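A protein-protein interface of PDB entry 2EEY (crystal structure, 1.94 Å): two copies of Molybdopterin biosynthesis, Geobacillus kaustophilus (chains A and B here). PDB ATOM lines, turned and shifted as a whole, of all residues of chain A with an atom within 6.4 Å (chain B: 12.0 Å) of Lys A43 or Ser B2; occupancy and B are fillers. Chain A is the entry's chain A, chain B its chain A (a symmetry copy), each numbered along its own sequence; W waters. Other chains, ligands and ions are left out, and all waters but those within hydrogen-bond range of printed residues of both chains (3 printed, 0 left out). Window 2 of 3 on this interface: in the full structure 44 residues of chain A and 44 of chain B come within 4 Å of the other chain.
Printed residues of chain B within 4 Å of Lys A43: Ser B2 (2.7 Å), Ser B3 (3.8 Å) and Phe B4 (3.9 Å). Glu A39 touches one residue of chain B. No residue of chain B comes within 4 Å of Glu A42. No residue of chain B comes within 4 Å of Ser A46. No residue of chain B comes within 4 Å of Asn A47. Glu A50 touches two residues of chain B. Of chain B, only Phe B7 (3.5 Å) and Gly B11 (3.3 Å) come within 4 Å of Gly A52. Ala A134 touches just one residue of chain B: Thr B5. Of chain B, only Ser B2 (3.6 Å), Ser B3 (3.6 Å) and Phe B4 (3.6 Å) come within 4 Å of Leu A135. Of the printed residues of chain A, Phe B4 touches Lys A43 (3.9 Å), Glu A50 (3.3 Å) and Leu A135 (3.6 Å). Of the printed residues of chain A, Ser B3 touches Lys A43 (3.8 Å), Glu A50 (2.5 Å) and Leu A135 (3.6 Å). The nearest residue of chain B that does not touch Lys A43 is Phe B7 (7.3 Å). The nearest residue of chain A that does not touch Ser B2 is Ala A134 (4.6 Å). The nearest printed residue of chain A that does not touch Phe B7 is Glu A50 (4.9 Å).
No position is printed for both chains. Of the 12 pairs that touch across the chains among the printed residues, none has its exchanged pair printed and touching as well.
Water W1 bridges the side-chain carboxylate (OE2) of Glu A50 (2.6 Å) and the backbone carbonyl oxygen (O) of Ser B2 (3.2 Å). Water W2 lies within hydrogen-bond range of N of Ala A134 (2.9 Å) and ND1 of His B6 (3.5 Å). Water W3 bridges the side-chain carboxylate (OE1) of Glu A50 (3.0 Å) and the backbone carbonyl oxygen (O) of Phe B4 (3.5 Å).
N of Phe B4 lies within hydrogen-bond range of OE2 of Glu A50, at 3.3 Å. The side-chain carboxylate (OE2) of Glu A50 sits at hydrogen-bond distance from the side-chain hydroxyl (OG) of Ser B3. The side-chain amino group (NZ) of Lys A43 is in hydrogen-bond range of the backbone carbonyl oxygen (O) of Ser B2.
The side-chain carboxylate (OE2) of Glu A39 lies within salt-bridge range of the side-chain amino group (NZ) of Lys A43. The side-chain hydroxyl of Thr B5 lies within hydrogen-bond range of a ring nitrogen (ND1) of His B6 (2.9 Å). The side-chain amide nitrogen (ND2) of Asn A47 is in hydrogen-bond range of the backbone carbonyl oxygen (O) of Glu A50, 3.4 Å away.
Glu A39 touches Ser B2. NZ of Lys A43 touches N of Ser B3, at 3.8 Å. Phe B4 touches Lys A43. Phe B7 touches Gly A52 (CE1 to CA, 3.5 Å). Gly A52 touches Gly B11. Ala A134 touches Thr B5. Ser B2 touches Leu A135. CD2 of Leu A135 touches N of Ser B3 (3.6 Å). Leu A135 touches Phe B4.
Of the 9 printed residues of chain B, 6 touch a printed residue of chain A. Hydrophobic or aromatic side chains of chain B within 4 Å of the printed part of chain A: Phe B4 and Phe B7. Among the printed residues, no Asp or Glu carboxylate lies within 4 Å of a Lys or Arg side-chain nitrogen of the other chain.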
ATOM      1  N   ARG A  38     -16.573 -13.286 -28.945  1.00  0.00           N
ATOM      2  CA  ARG A  38     -16.462 -11.917 -29.440  1.00  0.00           C
ATOM      3  C   ARG A  38     -17.347 -10.976 -28.633  1.00  0.00           C
ATOM      4  O   ARG A  38     -16.948  -9.855 -28.327  1.00  0.00           O
ATOM      5  CB  ARG A  38     -16.839 -11.842 -30.925  1.00  0.00           C
ATOM      6  CG  ARG A  38     -16.789 -10.425 -31.498  1.00  0.00           C
ATOM      7  CD  ARG A  38     -16.751 -10.419 -33.024  1.00  0.00           C
ATOM      8  NE  ARG A  38     -17.938 -11.015 -33.633  1.00  0.00           N
ATOM      9  CZ  ARG A  38     -19.148 -10.458 -33.635  1.00  0.00           C
ATOM     10  NH1 ARG A  38     -19.346  -9.281 -33.060  1.00  0.00           N
ATOM     11  NH2 ARG A  38     -20.162 -11.083 -34.221  1.00  0.00           N
ATOM     12  N   GLU A  39     -18.546 -11.434 -28.282  1.00  0.00           N
ATOM     13  CA  GLU A  39     -19.470 -10.612 -27.510  1.00  0.00           C
ATOM     14  C   GLU A  39     -18.886 -10.203 -26.163  1.00  0.00           C
ATOM     15  O   GLU A  39     -18.990  -9.046 -25.756  1.00  0.00           O
ATOM     16  CB  GLU A  39     -20.795 -11.349 -27.293  1.00  0.00           C
ATOM     17  CG  GLU A  39     -21.711 -10.652 -26.301  1.00  0.00           C
ATOM     18  CD  GLU A  39     -23.065 -11.323 -26.172  1.00  0.00           C
ATOM     19  OE1 GLU A  39     -23.114 -12.570 -26.116  1.00  0.00           O
ATOM     20  OE2 GLU A  39     -24.081 -10.600 -26.113  1.00  0.00           O
ATOM     21  N   ILE A  40     -18.272 -11.153 -25.466  1.00  0.00           N
ATOM     22  CA  ILE A  40     -17.669 -10.850 -24.172  1.00  0.00           C
ATOM     23  C   ILE A  40     -16.528  -9.844 -24.335  1.00  0.00           C
ATOM     24  O   ILE A  40     -16.405  -8.900 -23.554  1.00  0.00           O
ATOM     25  CB  ILE A  40     -17.151 -12.131 -23.490  1.00  0.00           C
ATOM     26  CG1 ILE A  40     -18.343 -12.912 -22.916  1.00  0.00           C
ATOM     27  CG2 ILE A  40     -16.147 -11.774 -22.390  1.00  0.00           C
ATOM     28  CD1 ILE A  40     -17.976 -14.261 -22.322  1.00  0.00           C
ATOM     29  N   TYR A  41     -15.699 -10.038 -25.354  1.00  0.00           N
ATOM     30  CA  TYR A  41     -14.595  -9.118 -25.601  1.00  0.00           C
ATOM     31  C   TYR A  41     -15.137  -7.708 -25.867  1.00  0.00           C
ATOM     32  O   TYR A  41     -14.633  -6.723 -25.331  1.00  0.00           O
ATOM     33  CB  TYR A  41     -13.774  -9.577 -26.812  1.00  0.00           C
ATOM     34  CG  TYR A  41     -12.773  -8.543 -27.270  1.00  0.00           C
ATOM     35  CD1 TYR A  41     -11.584  -8.336 -26.571  1.00  0.00           C
ATOM     36  CD2 TYR A  41     -13.048  -7.718 -28.367  1.00  0.00           C
ATOM     37  CE1 TYR A  41     -10.693  -7.328 -26.944  1.00  0.00           C
ATOM     38  CE2 TYR A  41     -12.167  -6.707 -28.746  1.00  0.00           C
ATOM     39  CZ  TYR A  41     -10.995  -6.515 -28.030  1.00  0.00           C
ATOM     40  OH  TYR A  41     -10.142  -5.493 -28.376  1.00  0.00           O
ATOM     41  N   GLU A  42     -16.175  -7.624 -26.694  1.00  0.00           N
ATOM     42  CA  GLU A  42     -16.771  -6.335 -27.044  1.00  0.00           C
ATOM     43  C   GLU A  42     -17.318  -5.585 -25.838  1.00  0.00           C
ATOM     44  O   GLU A  42     -17.119  -4.375 -25.705  1.00  0.00           O
ATOM     45  CB  GLU A  42     -17.891  -6.534 -28.075  1.00  0.00           C
ATOM     46  CG  GLU A  42     -17.404  -7.130 -29.387  1.00  0.00           C
ATOM     47  CD  GLU A  42     -18.527  -7.456 -30.353  1.00  0.00           C
ATOM     48  OE1 GLU A  42     -19.662  -7.724 -29.903  1.00  0.00           O
ATOM     49  OE2 GLU A  42     -18.264  -7.469 -31.570  1.00  0.00           O
ATOM     50  N   LYS A  43     -18.004  -6.294 -24.949  1.00  0.00           N
ATOM     51  CA  LYS A  43     -18.573  -5.634 -23.788  1.00  0.00           C
ATOM     52  C   LYS A  43     -17.541  -5.269 -22.733  1.00  0.00           C
ATOM     53  O   LYS A  43     -17.758  -4.351 -21.944  1.00  0.00           O
ATOM     54  CB  LYS A  43     -19.702  -6.488 -23.206  1.00  0.00           C
ATOM     55  CG  LYS A  43     -20.890  -6.530 -24.162  1.00  0.00           C
ATOM     56  CD  LYS A  43     -22.032  -7.411 -23.708  1.00  0.00           C
ATOM     57  CE  LYS A  43     -23.137  -7.391 -24.766  1.00  0.00           C
ATOM     58  NZ  LYS A  43     -24.275  -8.290 -24.430  1.00  0.00           N
ATOM     59  N   MET A  44     -16.410  -5.966 -22.732  1.00  0.00           N
ATOM     60  CA  MET A  44     -15.351  -5.671 -21.774  1.00  0.00           C
ATOM     61  C   MET A  44     -14.438  -4.550 -22.265  1.00  0.00           C
ATOM     62  O   MET A  44     -13.724  -3.939 -21.473  1.00  0.00           O
ATOM     63  CB  MET A  44     -14.498  -6.913 -21.513  1.00  0.00           C
ATOM     64  CG  MET A  44     -15.062  -7.875 -20.488  1.00  0.00           C
ATOM     65  SD  MET A  44     -13.923  -9.258 -20.252  1.00  0.00           S
ATOM     66  CE  MET A  44     -12.691  -8.495 -19.260  1.00  0.00           C
ATOM     67  N   THR A  45     -14.457  -4.273 -23.564  1.00  0.00           N
ATOM     68  CA  THR A  45     -13.583  -3.235 -24.100  1.00  0.00           C
ATOM     69  C   THR A  45     -14.275  -1.940 -24.515  1.00  0.00           C
ATOM     70  O   THR A  45     -13.630  -1.034 -25.043  1.00  0.00           O
ATOM     71  CB  THR A  45     -12.757  -3.772 -25.285  1.00  0.00           C
ATOM     72  OG1 THR A  45     -13.632  -4.297 -26.286  1.00  0.00           O
ATOM     73  CG2 THR A  45     -11.822  -4.882 -24.816  1.00  0.00           C
ATOM     74  N   SER A  46     -15.579  -1.849 -24.275  1.00  0.00           N
ATOM     75  CA  SER A  46     -16.331  -0.640 -24.601  1.00  0.00           C
ATOM     76  C   SER A  46     -17.138  -0.180 -23.393  1.00  0.00           C
ATOM     77  O   SER A  46     -17.746  -0.992 -22.705  1.00  0.00           O
ATOM     78  CB  SER A  46     -17.285  -0.886 -25.770  1.00  0.00           C
ATOM     79  OG  SER A  46     -18.081   0.268 -26.010  1.00  0.00           O
ATOM     80  N   ASN A  47     -17.145   1.125 -23.141  1.00  0.00           N
ATOM     81  CA  ASN A  47     -17.894   1.685 -22.019  1.00  0.00           C
ATOM     82  C   ASN A  47     -19.185   2.346 -22.488  1.00  0.00           C
ATOM     83  O   ASN A  47     -19.865   3.021 -21.713  1.00  0.00           O
ATOM     84  CB  ASN A  47     -17.040   2.711 -21.266  1.00  0.00           C
ATOM     85  CG  ASN A  47     -16.075   2.066 -20.291  1.00  0.00           C
ATOM     86  OD1 ASN A  47     -15.216   2.736 -19.722  1.00  0.00           O
ATOM     87  ND2 ASN A  47     -16.220   0.761 -20.086  1.00  0.00           N
ATOM     88  N   GLU A  50     -21.983  -0.922 -21.011  1.00  0.00           N
ATOM     89  CA  GLU A  50     -21.524  -1.575 -19.787  1.00  0.00           C
ATOM     90  C   GLU A  50     -20.333  -0.777 -19.267  1.00  0.00           C
ATOM     91  O   GLU A  50     -19.252  -0.818 -19.850  1.00  0.00           O
ATOM     92  CB  GLU A  50     -21.081  -3.013 -20.076  1.00  0.00           C
ATOM     93  CG  GLU A  50     -22.166  -3.928 -20.628  1.00  0.00           C
ATOM     94  CD  GLU A  50     -23.261  -4.231 -19.617  1.00  0.00           C
ATOM     95  OE1 GLU A  50     -23.090  -3.904 -18.422  1.00  0.00           O
ATOM     96  OE2 GLU A  50     -24.293  -4.809 -20.019  1.00  0.00           O
ATOM     97  N   LYS A  51     -20.525  -0.051 -18.172  1.00  0.00           N
ATOM     98  CA  LYS A  51     -19.438   0.747 -17.623  1.00  0.00           C
ATOM     99  C   LYS A  51     -18.672   0.010 -16.526  1.00  0.00           C
ATOM    100  O   LYS A  51     -17.627   0.469 -16.074  1.00  0.00           O
ATOM    101  CB  LYS A  51     -19.991   2.080 -17.114  1.00  0.00           C
ATOM    102  CG  LYS A  51     -20.767   2.832 -18.200  1.00  0.00           C
ATOM    103  CD  LYS A  51     -21.277   4.183 -17.740  1.00  0.00           C
ATOM    104  CE  LYS A  51     -22.176   4.813 -18.801  1.00  0.00           C
ATOM    105  NZ  LYS A  51     -21.494   4.936 -20.128  1.00  0.00           N
ATOM    106  N   GLY A  52     -19.183  -1.148 -16.121  1.00  0.00           N
ATOM    107  CA  GLY A  52     -18.518  -1.924 -15.087  1.00  0.00           C
ATOM    108  C   GLY A  52     -17.145  -2.410 -15.522  1.00  0.00           C
ATOM    109  O   GLY A  52     -16.971  -2.871 -16.651  1.00  0.00           O
ATOM    110  N   ALA A 134     -22.580 -14.746 -17.517  1.00  0.00           N
ATOM    111  CA  ALA A 134     -23.971 -14.463 -17.860  1.00  0.00           C
ATOM    112  C   ALA A 134     -24.094 -14.363 -19.381  1.00  0.00           C
ATOM    113  O   ALA A 134     -25.144 -14.666 -19.951  1.00  0.00           O
ATOM    114  CB  ALA A 134     -24.422 -13.160 -17.207  1.00  0.00           C
ATOM    115  N   LEU A 135     -23.009 -13.951 -20.032  1.00  0.00           N
ATOM    116  CA  LEU A 135     -22.985 -13.801 -21.486  1.00  0.00           C
ATOM    117  C   LEU A 135     -22.647 -15.101 -22.218  1.00  0.00           C
ATOM    118  O   LEU A 135     -23.192 -15.378 -23.286  1.00  0.00           O
ATOM    119  CB  LEU A 135     -21.974 -12.717 -21.882  1.00  0.00           C
ATOM    120  CG  LEU A 135     -22.146 -11.333 -21.245  1.00  0.00           C
ATOM    121  CD1 LEU A 135     -21.009 -10.423 -21.677  1.00  0.00           C
ATOM    122  CD2 LEU A 135     -23.478 -10.739 -21.661  1.00  0.00           C
ATOM    123  N   SER B   2     -28.516  -9.086 -24.514  1.00  0.00           N
ATOM    124  CA  SER B   2     -27.687  -9.694 -23.480  1.00  0.00           C
ATOM    125  C   SER B   2     -26.893  -8.643 -22.710  1.00  0.00           C
ATOM    126  O   SER B   2     -26.568  -7.570 -23.210  1.00  0.00           O
ATOM    127  CB  SER B   2     -26.725 -10.676 -24.154  1.00  0.00           C
ATOM    128  OG  SER B   2     -26.522 -11.790 -23.294  1.00  0.00           O
ATOM    129  N   SER B   3     -26.610  -8.910 -21.439  1.00  0.00           N
ATOM    130  CA  SER B   3     -25.940  -7.926 -20.595  1.00  0.00           C
ATOM    131  C   SER B   3     -25.360  -8.543 -19.326  1.00  0.00           C
ATOM    132  O   SER B   3     -25.769  -9.628 -18.908  1.00  0.00           O
ATOM    133  CB  SER B   3     -26.935  -6.821 -20.219  1.00  0.00           C
ATOM    134  OG  SER B   3     -26.415  -5.955 -19.224  1.00  0.00           O
ATOM    135  N   PHE B   4     -24.402  -7.847 -18.720  1.00  0.00           N
ATOM    136  CA  PHE B   4     -23.809  -8.315 -17.470  1.00  0.00           C
ATOM    137  C   PHE B   4     -24.875  -8.294 -16.379  1.00  0.00           C
ATOM    138  O   PHE B   4     -25.821  -7.515 -16.418  1.00  0.00           O
ATOM    139  CB  PHE B   4     -22.652  -7.373 -17.063  1.00  0.00           C
ATOM    140  CG  PHE B   4     -21.437  -7.522 -17.952  1.00  0.00           C
ATOM    141  CD1 PHE B   4     -20.774  -8.745 -18.041  1.00  0.00           C
ATOM    142  CD2 PHE B   4     -20.910  -6.397 -18.563  1.00  0.00           C
ATOM    143  CE1 PHE B   4     -19.598  -8.835 -18.781  1.00  0.00           C
ATOM    144  CE2 PHE B   4     -19.734  -6.497 -19.302  1.00  0.00           C
ATOM    145  CZ  PHE B   4     -19.082  -7.718 -19.428  1.00  0.00           C
ATOM    146  N   THR B   5     -24.741  -9.218 -15.416  1.00  0.00           N
ATOM    147  CA  THR B   5     -25.667  -9.205 -14.285  1.00  0.00           C
ATOM    148  C   THR B   5     -24.963  -8.795 -12.976  1.00  0.00           C
ATOM    149  O   THR B   5     -25.593  -8.504 -11.968  1.00  0.00           O
ATOM    150  CB  THR B   5     -26.257 -10.610 -14.133  1.00  0.00           C
ATOM    151  OG1 THR B   5     -25.195 -11.545 -13.926  1.00  0.00           O
ATOM    152  CG2 THR B   5     -27.042 -11.017 -15.388  1.00  0.00           C
ATOM    153  N   HIS B   6     -23.611  -8.827 -13.010  1.00  0.00           N
ATOM    154  CA  HIS B   6     -22.829  -8.630 -11.786  1.00  0.00           C
ATOM    155  C   HIS B   6     -22.441  -7.160 -11.572  1.00  0.00           C
ATOM    156  O   HIS B   6     -21.604  -6.829 -10.744  1.00  0.00           O
ATOM    157  CB  HIS B   6     -21.569  -9.493 -11.896  1.00  0.00           C
ATOM    158  CG  HIS B   6     -21.887 -10.939 -11.614  1.00  0.00           C
ATOM    159  ND1 HIS B   6     -22.984 -11.563 -12.098  1.00  0.00           N
ATOM    160  CD2 HIS B   6     -21.140 -11.857 -10.872  1.00  0.00           C
ATOM    161  CE1 HIS B   6     -22.898 -12.832 -11.662  1.00  0.00           C
ATOM    162  NE2 HIS B   6     -21.806 -13.039 -10.926  1.00  0.00           N
ATOM    163  N   PHE B   7     -23.049  -6.219 -12.287  1.00  0.00           N
ATOM    164  CA  PHE B   7     -22.758  -4.800 -12.074  1.00  0.00           C
ATOM    165  C   PHE B   7     -24.044  -4.064 -11.705  1.00  0.00           C
ATOM    166  O   PHE B   7     -25.117  -4.388 -12.214  1.00  0.00           O
ATOM    167  CB  PHE B   7     -22.134  -4.177 -13.327  1.00  0.00           C
ATOM    168  CG  PHE B   7     -20.719  -4.621 -13.584  1.00  0.00           C
ATOM    169  CD1 PHE B   7     -19.687  -4.232 -12.734  1.00  0.00           C
ATOM    170  CD2 PHE B   7     -20.418  -5.433 -14.672  1.00  0.00           C
ATOM    171  CE1 PHE B   7     -18.375  -4.646 -12.963  1.00  0.00           C
ATOM    172  CE2 PHE B   7     -19.107  -5.853 -14.910  1.00  0.00           C
ATOM    173  CZ  PHE B   7     -18.086  -5.457 -14.054  1.00  0.00           C
ATOM    174  N   GLY B  11     -22.351   1.044 -12.065  1.00  0.00           N
ATOM    175  CA  GLY B  11     -21.245   0.431 -12.779  1.00  0.00           C
ATOM    176  C   GLY B  11     -20.219  -0.263 -11.897  1.00  0.00           C
ATOM    177  O   GLY B  11     -19.054  -0.380 -12.270  1.00  0.00           O
ATOM    178  N   LYS B 153     -32.279 -21.151 -15.320  1.00  0.00           N
ATOM    179  CA  LYS B 153     -32.880 -20.498 -16.479  1.00  0.00           C
ATOM    180  C   LYS B 153     -32.311 -20.974 -17.813  1.00  0.00           C
ATOM    181  O   LYS B 153     -33.036 -21.514 -18.650  1.00  0.00           O
ATOM    182  CB  LYS B 153     -32.693 -18.982 -16.358  1.00  0.00           C
ATOM    183  CG  LYS B 153     -33.041 -18.185 -17.605  1.00  0.00           C
ATOM    184  CD  LYS B 153     -32.624 -16.732 -17.437  1.00  0.00           C
ATOM    185  CE  LYS B 153     -32.830 -15.931 -18.712  1.00  0.00           C
ATOM    186  NZ  LYS B 153     -32.336 -14.531 -18.569  1.00  0.00           N
ATOM    187  N   SER B 154     -31.011 -20.766 -18.003  1.00  0.00           N
ATOM    188  CA  SER B 154     -30.326 -21.146 -19.235  1.00  0.00           C
ATOM    189  C   SER B 154     -30.411 -22.634 -19.567  1.00  0.00           C
ATOM    190  O   SER B 154     -29.711 -23.117 -20.459  1.00  0.00           O
ATOM    191  CB  SER B 154     -28.859 -20.718 -19.164  1.00  0.00           C
ATOM    192  OG  SER B 154     -28.229 -21.244 -18.009  1.00  0.00           O
HETATM  193  O   HOH W   1     -24.973  -4.846 -22.479  1.00  0.00           O
HETATM  194  O   HOH W   2     -22.246 -13.399 -14.935  1.00  0.00           O
HETATM  195  O   HOH W   3     -25.133  -4.093 -16.297  1.00  0.00           O
